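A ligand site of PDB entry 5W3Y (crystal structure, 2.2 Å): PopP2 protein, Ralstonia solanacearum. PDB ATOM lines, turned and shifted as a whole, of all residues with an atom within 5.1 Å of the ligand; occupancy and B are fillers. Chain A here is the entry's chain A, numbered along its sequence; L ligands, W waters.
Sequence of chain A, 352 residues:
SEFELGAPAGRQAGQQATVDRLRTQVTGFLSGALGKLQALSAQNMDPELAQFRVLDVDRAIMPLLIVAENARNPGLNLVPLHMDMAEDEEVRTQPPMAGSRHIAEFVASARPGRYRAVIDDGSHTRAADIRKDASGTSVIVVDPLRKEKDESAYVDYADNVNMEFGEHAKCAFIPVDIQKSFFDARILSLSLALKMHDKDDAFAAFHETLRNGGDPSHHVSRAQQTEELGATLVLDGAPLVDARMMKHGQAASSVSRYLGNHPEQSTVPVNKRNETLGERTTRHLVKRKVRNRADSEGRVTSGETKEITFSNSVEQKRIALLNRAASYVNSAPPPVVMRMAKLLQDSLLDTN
An oxygen (O22) of the ligand is in salt-bridge range of the side-chain amino group (NZ) of Lys 272 (2.9 Å).
An oxygen (O22) of the ligand is in hydrogen-bond range of the backbone NH (N) of Lys 272, 2.8 Å away.
NZ of Lys 247 lies within salt-bridge range of O2 of the ligand.
An oxygen (O8) of the ligand is in salt-bridge range of the side-chain amino group (NZ) of Lys 195 (2.6 Å).
An oxygen (O3) of the ligand is in salt-bridge range of the guanidinium group (NH2) of Arg 280, at 2.7 Å.
The guanidinium group (NH2) of Arg 72 is in salt-bridge range of an oxygen (O12) of the ligand, 2.7 Å away.
The side-chain amide nitrogen of Asn 271 lies within hydrogen-bond range of an oxygen (O2) of the ligand, at 2.9 Å.
NH2 of Arg 244 lies within salt-bridge range of O14 of the ligand.
O7 of the ligand lies within hydrogen-bond range of NE2 of His 248 (2.7 Å).
The guanidinium group of Arg 324 lies within salt-bridge range of an oxygen (O11) of the ligand, 2.4 Å away.
The side-chain amino group of Lys 317 is in salt-bridge range of an oxygen (O7) of the ligand (2.8 Å).
OG of Ser 191 sits close to NE2 of His 248, at 3.3 Å.
N of Arg 273 sits close to OD1 of Asn 271.
NH1 of Arg 244 is in salt-bridge range of OD2 of Asp 198.
The side-chain carboxylate (OE1) of Glu 69 lies within salt-bridge range of the guanidinium group (NE) of Arg 72, at 2.8 Å.
O of Val 270 is in hydrogen-bond range of NE of Arg 244, 3.2 Å away.
O of Val 270 lies within hydrogen-bond range of NZ of Lys 247 (3.1 Å).
The side-chain carboxylate (OE2) of Glu 69 lies within salt-bridge range of the guanidinium group (NH2) of Arg 324 (3.0 Å).
Merely in contact with the ligand: Leu 194 (3.3 Å).
Hydrophobic or aromatic side chains that line the ligand: Leu 194 and His 248.
Within 4 Å of the ligand: Arg 72, Leu 194, Lys 195, Arg 244, Lys 247, His 248, Asn 271, Lys 272, Arg 280, Lys 317 and Arg 324.
The nearest printed residue that does not touch the ligand is Ser 191 (4.1 Å).
Water W1 lies within hydrogen-bond range of an oxygen (O10) of the ligand (2.6 Å), the side-chain hydroxyl of Ser 191 (3.1 Å) and the side-chain amino group of Lys 317 (3.4 Å).
Water W2 bridges an oxygen (O4) of the ligand (2.8 Å) and the guanidinium group (NH2) of Arg 283 (3.1 Å).
Water W3 bridges O10 of the ligand (2.8 Å) and O of Leu 194 (3.3 Å).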
ATOM      1  N   GLU A  69      30.426 -26.541   4.487  1.00  0.00           N
ATOM      2  CA  GLU A  69      29.044 -26.344   4.911  1.00  0.00           C
ATOM      3  C   GLU A  69      28.601 -27.404   5.938  1.00  0.00           C
ATOM      4  O   GLU A  69      27.853 -27.084   6.881  1.00  0.00           O
ATOM      5  CB  GLU A  69      28.116 -26.344   3.706  1.00  0.00           C
ATOM      6  CG  GLU A  69      28.323 -25.138   2.777  1.00  0.00           C
ATOM      7  CD  GLU A  69      28.219 -23.808   3.488  1.00  0.00           C
ATOM      8  OE1 GLU A  69      27.383 -23.679   4.414  1.00  0.00           O
ATOM      9  OE2 GLU A  69      28.972 -22.884   3.144  1.00  0.00           O
ATOM     10  N   ARG A  72      30.049 -26.205   9.071  1.00  0.00           N
ATOM     11  CA  ARG A  72      29.457 -24.932   9.460  1.00  0.00           C
ATOM     12  C   ARG A  72      28.042 -25.154  10.026  1.00  0.00           C
ATOM     13  O   ARG A  72      27.601 -24.419  10.914  1.00  0.00           O
ATOM     14  CB  ARG A  72      29.415 -23.977   8.261  1.00  0.00           C
ATOM     15  CG  ARG A  72      28.908 -22.577   8.585  1.00  0.00           C
ATOM     16  CD  ARG A  72      28.921 -21.662   7.358  1.00  0.00           C
ATOM     17  NE  ARG A  72      27.708 -21.857   6.557  1.00  0.00           N
ATOM     18  CZ  ARG A  72      26.588 -21.142   6.698  1.00  0.00           C
ATOM     19  NH1 ARG A  72      26.531 -20.165   7.584  1.00  0.00           N
ATOM     20  NH2 ARG A  72      25.541 -21.417   5.936  1.00  0.00           N
ATOM     21  N   SER A 191      22.676 -24.419  -2.589  1.00  0.00           N
ATOM     22  CA  SER A 191      21.885 -23.445  -1.861  1.00  0.00           C
ATOM     23  C   SER A 191      20.537 -24.028  -1.435  1.00  0.00           C
ATOM     24  O   SER A 191      20.098 -23.834  -0.301  1.00  0.00           O
ATOM     25  CB  SER A 191      21.679 -22.187  -2.715  1.00  0.00           C
ATOM     26  OG  SER A 191      20.742 -21.319  -2.112  1.00  0.00           O
ATOM     27  N   LEU A 194      20.918 -26.334   1.542  1.00  0.00           N
ATOM     28  CA  LEU A 194      21.088 -25.578   2.783  1.00  0.00           C
ATOM     29  C   LEU A 194      19.756 -25.100   3.328  1.00  0.00           C
ATOM     30  O   LEU A 194      19.540 -25.076   4.539  1.00  0.00           O
ATOM     31  CB  LEU A 194      22.009 -24.381   2.568  1.00  0.00           C
ATOM     32  CG  LEU A 194      23.454 -24.647   2.178  1.00  0.00           C
ATOM     33  CD1 LEU A 194      24.146 -23.322   1.938  1.00  0.00           C
ATOM     34  CD2 LEU A 194      24.186 -25.457   3.235  1.00  0.00           C
ATOM     35  N   LYS A 195      18.891 -24.681   2.410  1.00  0.00           N
ATOM     36  CA  LYS A 195      17.570 -24.221   2.753  1.00  0.00           C
ATOM     37  C   LYS A 195      16.713 -25.381   3.281  1.00  0.00           C
ATOM     38  O   LYS A 195      15.857 -25.191   4.138  1.00  0.00           O
ATOM     39  CB  LYS A 195      16.906 -23.554   1.560  1.00  0.00           C
ATOM     40  CG  LYS A 195      17.505 -22.202   1.159  1.00  0.00           C
ATOM     41  CD  LYS A 195      17.805 -21.319   2.371  1.00  0.00           C
ATOM     42  CE  LYS A 195      18.306 -19.960   1.912  1.00  0.00           C
ATOM     43  NZ  LYS A 195      19.253 -19.308   2.852  1.00  0.00           N
ATOM     44  N   ASP A 198      17.559 -25.754   6.710  1.00  0.00           N
ATOM     45  CA  ASP A 198      16.946 -24.614   7.372  1.00  0.00           C
ATOM     46  C   ASP A 198      15.458 -24.884   7.637  1.00  0.00           C
ATOM     47  O   ASP A 198      14.915 -24.525   8.687  1.00  0.00           O
ATOM     48  CB  ASP A 198      17.128 -23.360   6.536  1.00  0.00           C
ATOM     49  CG  ASP A 198      16.862 -22.092   7.314  1.00  0.00           C
ATOM     50  OD1 ASP A 198      17.417 -21.961   8.428  1.00  0.00           O
ATOM     51  OD2 ASP A 198      16.127 -21.220   6.818  1.00  0.00           O
ATOM     52  N   ARG A 244      12.159 -17.840   0.590  1.00  0.00           N
ATOM     53  CA  ARG A 244      13.581 -18.017   0.836  1.00  0.00           C
ATOM     54  C   ARG A 244      14.223 -18.993  -0.144  1.00  0.00           C
ATOM     55  O   ARG A 244      15.401 -18.882  -0.444  1.00  0.00           O
ATOM     56  CB  ARG A 244      13.841 -18.458   2.280  1.00  0.00           C
ATOM     57  CG  ARG A 244      13.919 -17.281   3.263  1.00  0.00           C
ATOM     58  CD  ARG A 244      14.085 -17.693   4.725  1.00  0.00           C
ATOM     59  NE  ARG A 244      15.331 -17.135   5.246  1.00  0.00           N
ATOM     60  CZ  ARG A 244      16.514 -17.740   5.216  1.00  0.00           C
ATOM     61  NH1 ARG A 244      16.620 -18.966   4.707  1.00  0.00           N
ATOM     62  NH2 ARG A 244      17.593 -17.130   5.686  1.00  0.00           N
ATOM     63  N   LYS A 247      15.052 -17.159  -3.581  1.00  0.00           N
ATOM     64  CA  LYS A 247      15.972 -16.019  -3.511  1.00  0.00           C
ATOM     65  C   LYS A 247      16.879 -15.872  -4.724  1.00  0.00           C
ATOM     66  O   LYS A 247      17.076 -14.767  -5.225  1.00  0.00           O
ATOM     67  CB  LYS A 247      16.813 -16.131  -2.260  1.00  0.00           C
ATOM     68  CG  LYS A 247      16.054 -15.882  -1.007  1.00  0.00           C
ATOM     69  CD  LYS A 247      16.789 -14.880  -0.202  1.00  0.00           C
ATOM     70  CE  LYS A 247      17.371 -15.514   0.974  1.00  0.00           C
ATOM     71  NZ  LYS A 247      18.369 -14.608   1.524  1.00  0.00           N
ATOM     72  N   HIS A 248      17.421 -16.982  -5.203  1.00  0.00           N
ATOM     73  CA  HIS A 248      18.420 -16.920  -6.263  1.00  0.00           C
ATOM     74  C   HIS A 248      17.822 -17.042  -7.662  1.00  0.00           C
ATOM     75  O   HIS A 248      18.526 -17.375  -8.621  1.00  0.00           O
ATOM     76  CB  HIS A 248      19.492 -17.999  -6.024  1.00  0.00           C
ATOM     77  CG  HIS A 248      20.167 -17.862  -4.693  1.00  0.00           C
ATOM     78  ND1 HIS A 248      20.825 -16.704  -4.316  1.00  0.00           N
ATOM     79  CD2 HIS A 248      20.292 -18.721  -3.658  1.00  0.00           C
ATOM     80  CE1 HIS A 248      21.317 -16.858  -3.096  1.00  0.00           C
ATOM     81  NE2 HIS A 248      21.001 -18.062  -2.676  1.00  0.00           N
ATOM     82  N   VAL A 270      13.281 -12.381   3.871  1.00  0.00           N
ATOM     83  CA  VAL A 270      14.063 -13.511   3.356  1.00  0.00           C
ATOM     84  C   VAL A 270      15.462 -13.544   3.953  1.00  0.00           C
ATOM     85  O   VAL A 270      16.215 -14.484   3.731  1.00  0.00           O
ATOM     86  CB  VAL A 270      14.179 -13.459   1.798  1.00  0.00           C
ATOM     87  CG1 VAL A 270      12.816 -13.672   1.150  1.00  0.00           C
ATOM     88  CG2 VAL A 270      14.795 -12.151   1.319  1.00  0.00           C
ATOM     89  N   ASN A 271      15.820 -12.489   4.683  1.00  0.00           N
ATOM     90  CA  ASN A 271      17.100 -12.469   5.365  1.00  0.00           C
ATOM     91  C   ASN A 271      17.060 -11.598   6.614  1.00  0.00           C
ATOM     92  O   ASN A 271      16.024 -11.029   6.955  1.00  0.00           O
ATOM     93  CB  ASN A 271      18.213 -12.001   4.426  1.00  0.00           C
ATOM     94  CG  ASN A 271      17.905 -10.672   3.754  1.00  0.00           C
ATOM     95  OD1 ASN A 271      17.201  -9.817   4.321  1.00  0.00           O
ATOM     96  ND2 ASN A 271      18.398 -10.506   2.532  1.00  0.00           N
ATOM     97  N   LYS A 272      18.188 -11.522   7.311  1.00  0.00           N
ATOM     98  CA  LYS A 272      18.272 -10.781   8.548  1.00  0.00           C
ATOM     99  C   LYS A 272      18.258  -9.271   8.358  1.00  0.00           C
ATOM    100  O   LYS A 272      18.042  -8.527   9.306  1.00  0.00           O
ATOM    101  CB  LYS A 272      19.523 -11.199   9.342  1.00  0.00           C
ATOM    102  CG  LYS A 272      19.411 -12.573  10.003  1.00  0.00           C
ATOM    103  CD  LYS A 272      20.564 -12.844  10.975  1.00  0.00           C
ATOM    104  CE  LYS A 272      21.882 -13.017  10.233  1.00  0.00           C
ATOM    105  NZ  LYS A 272      21.816 -14.084   9.174  1.00  0.00           N
ATOM    106  N   ARG A 273      18.513  -8.804   7.144  1.00  0.00           N
ATOM    107  CA  ARG A 273      18.423  -7.377   6.876  1.00  0.00           C
ATOM    108  C   ARG A 273      16.957  -6.955   6.624  1.00  0.00           C
ATOM    109  O   ARG A 273      16.689  -5.796   6.320  1.00  0.00           O
ATOM    110  CB  ARG A 273      19.358  -6.979   5.737  1.00  0.00           C
ATOM    111  CG  ARG A 273      18.860  -7.144   4.362  1.00  0.00           C
ATOM    112  CD  ARG A 273      19.834  -6.457   3.412  1.00  0.00           C
ATOM    113  NE  ARG A 273      21.196  -6.959   3.564  1.00  0.00           N
ATOM    114  CZ  ARG A 273      22.236  -6.552   2.829  1.00  0.00           C
ATOM    115  NH1 ARG A 273      22.075  -5.615   1.905  1.00  0.00           N
ATOM    116  NH2 ARG A 273      23.435  -7.073   3.041  1.00  0.00           N
ATOM    117  N   ARG A 280      15.004  -7.827  -2.416  1.00  0.00           N
ATOM    118  CA  ARG A 280      16.331  -8.427  -2.551  1.00  0.00           C
ATOM    119  C   ARG A 280      16.662  -8.671  -4.016  1.00  0.00           C
ATOM    120  O   ARG A 280      17.765  -8.341  -4.468  1.00  0.00           O
ATOM    121  CB  ARG A 280      16.434  -9.723  -1.768  1.00  0.00           C
ATOM    122  CG  ARG A 280      17.870 -10.277  -1.738  1.00  0.00           C
ATOM    123  CD  ARG A 280      17.952 -11.671  -1.135  1.00  0.00           C
ATOM    124  NE  ARG A 280      19.335 -12.136  -1.092  1.00  0.00           N
ATOM    125  CZ  ARG A 280      20.002 -12.598  -2.142  1.00  0.00           C
ATOM    126  NH1 ARG A 280      19.405 -12.647  -3.322  1.00  0.00           N
ATOM    127  NH2 ARG A 280      21.264 -12.997  -2.019  1.00  0.00           N
ATOM    128  N   ARG A 283      17.535  -5.519  -5.970  1.00  0.00           N
ATOM    129  CA  ARG A 283      18.894  -5.094  -5.618  1.00  0.00           C
ATOM    130  C   ARG A 283      19.972  -5.858  -6.425  1.00  0.00           C
ATOM    131  O   ARG A 283      21.094  -5.376  -6.582  1.00  0.00           O
ATOM    132  CB  ARG A 283      19.107  -5.261  -4.104  1.00  0.00           C
ATOM    133  CG  ARG A 283      20.505  -5.046  -3.619  1.00  0.00           C
ATOM    134  CD  ARG A 283      20.546  -4.854  -2.116  1.00  0.00           C
ATOM    135  NE  ARG A 283      20.282  -6.092  -1.378  1.00  0.00           N
ATOM    136  CZ  ARG A 283      21.194  -7.032  -1.148  1.00  0.00           C
ATOM    137  NH1 ARG A 283      22.422  -6.903  -1.616  1.00  0.00           N
ATOM    138  NH2 ARG A 283      20.863  -8.118  -0.445  1.00  0.00           N
ATOM    139  N   LYS A 317      26.391 -15.561  -4.668  1.00  0.00           N
ATOM    140  CA  LYS A 317      26.339 -16.676  -3.752  1.00  0.00           C
ATOM    141  C   LYS A 317      27.563 -17.566  -3.932  1.00  0.00           C
ATOM    142  O   LYS A 317      28.150 -18.022  -2.952  1.00  0.00           O
ATOM    143  CB  LYS A 317      25.061 -17.504  -3.950  1.00  0.00           C
ATOM    144  CG  LYS A 317      24.925 -18.631  -2.951  1.00  0.00           C
ATOM    145  CD  LYS A 317      24.679 -18.042  -1.547  1.00  0.00           C
ATOM    146  CE  LYS A 317      24.609 -19.098  -0.457  1.00  0.00           C
ATOM    147  NZ  LYS A 317      24.201 -18.505   0.853  1.00  0.00           N
ATOM    148  N   ARG A 324      33.358 -18.275   2.552  1.00  0.00           N
ATOM    149  CA  ARG A 324      33.120 -19.164   3.687  1.00  0.00           C
ATOM    150  C   ARG A 324      34.135 -20.276   3.735  1.00  0.00           C
ATOM    151  O   ARG A 324      34.754 -20.531   4.761  1.00  0.00           O
ATOM    152  CB  ARG A 324      31.734 -19.817   3.608  1.00  0.00           C
ATOM    153  CG  ARG A 324      30.570 -18.989   4.051  1.00  0.00           C
ATOM    154  CD  ARG A 324      29.350 -19.887   4.058  1.00  0.00           C
ATOM    155  NE  ARG A 324      28.135 -19.117   4.127  1.00  0.00           N
ATOM    156  CZ  ARG A 324      26.935 -19.583   3.800  1.00  0.00           C
ATOM    157  NH1 ARG A 324      25.886 -18.790   3.896  1.00  0.00           N
ATOM    158  NH2 ARG A 324      26.803 -20.841   3.391  1.00  0.00           N
HETATM  159  C1  LIG L   1      21.512 -14.783   3.877  1.00  0.00           C
HETATM  160  C2  LIG L   1      21.534 -16.286   3.368  1.00  0.00           C
HETATM  161  C3  LIG L   1      21.903 -17.460   4.322  1.00  0.00           C
HETATM  162  C4  LIG L   1      22.031 -16.941   5.798  1.00  0.00           C
HETATM  163  C5  LIG L   1      22.914 -15.704   6.047  1.00  0.00           C
HETATM  164  C6  LIG L   1      22.116 -14.576   5.332  1.00  0.00           C
HETATM  165  O1  LIG L   1      22.104 -14.030   3.040  1.00  0.00           O
HETATM  166  P1  LIG L   1      21.545 -12.930   1.922  1.00  0.00           P
HETATM  167  O2  LIG L   1      20.034 -12.758   1.875  1.00  0.00           O
HETATM  168  O3  LIG L   1      22.002 -13.356   0.510  1.00  0.00           O
HETATM  169  O4  LIG L   1      22.167 -11.568   2.231  1.00  0.00           O
HETATM  170  O5  LIG L   1      22.125 -16.423   2.137  1.00  0.00           O
HETATM  171  P2  LIG L   1      21.115 -16.787   0.847  1.00  0.00           P
HETATM  172  O6  LIG L   1      20.807 -15.576  -0.022  1.00  0.00           O
HETATM  173  O7  LIG L   1      21.625 -17.965  -0.001  1.00  0.00           O
HETATM  174  O8  LIG L   1      19.801 -17.242   1.443  1.00  0.00           O
HETATM  175  O9  LIG L   1      22.886 -18.172   3.880  1.00  0.00           O
HETATM  176  P3  LIG L   1      22.904 -19.842   3.996  1.00  0.00           P
HETATM  177  O10 LIG L   1      21.665 -20.514   3.401  1.00  0.00           O
HETATM  178  O11 LIG L   1      24.124 -20.329   3.205  1.00  0.00           O
HETATM  179  O12 LIG L   1      23.098 -20.307   5.429  1.00  0.00           O
HETATM  180  O13 LIG L   1      22.223 -17.914   6.696  1.00  0.00           O
HETATM  181  P4  LIG L   1      20.979 -18.655   7.470  1.00  0.00           P
HETATM  182  O14 LIG L   1      19.774 -18.648   6.535  1.00  0.00           O
HETATM  183  O15 LIG L   1      21.312 -20.122   7.864  1.00  0.00           O
HETATM  184  O16 LIG L   1      20.604 -17.925   8.780  1.00  0.00           O
HETATM  185  O17 LIG L   1      24.235 -15.746   5.826  1.00  0.00           O
HETATM  186  P5  LIG L   1      25.399 -14.984   6.871  1.00  0.00           P
HETATM  187  O18 LIG L   1      24.882 -14.973   8.312  1.00  0.00           O
HETATM  188  O19 LIG L   1      26.739 -15.747   6.861  1.00  0.00           O
HETATM  189  O20 LIG L   1      25.733 -13.533   6.482  1.00  0.00           O
HETATM  190  O21 LIG L   1      22.697 -13.386   5.420  1.00  0.00           O
HETATM  191  P6  LIG L   1      21.932 -12.138   6.147  1.00  0.00           P
HETATM  192  O22 LIG L   1      20.705 -12.708   6.862  1.00  0.00           O
HETATM  193  O23 LIG L   1      22.828 -11.422   7.189  1.00  0.00           O
HETATM  194  O24 LIG L   1      21.477 -11.088   5.130  1.00  0.00           O
HETATM  195  O   HOH W   1      21.701 -20.838   0.840  1.00  0.00           O
HETATM  196  O   HOH W   2      23.113 -10.123   0.044  1.00  0.00           O
HETATM  197  O   HOH W   3      20.103 -21.935   5.291  1.00  0.00           O
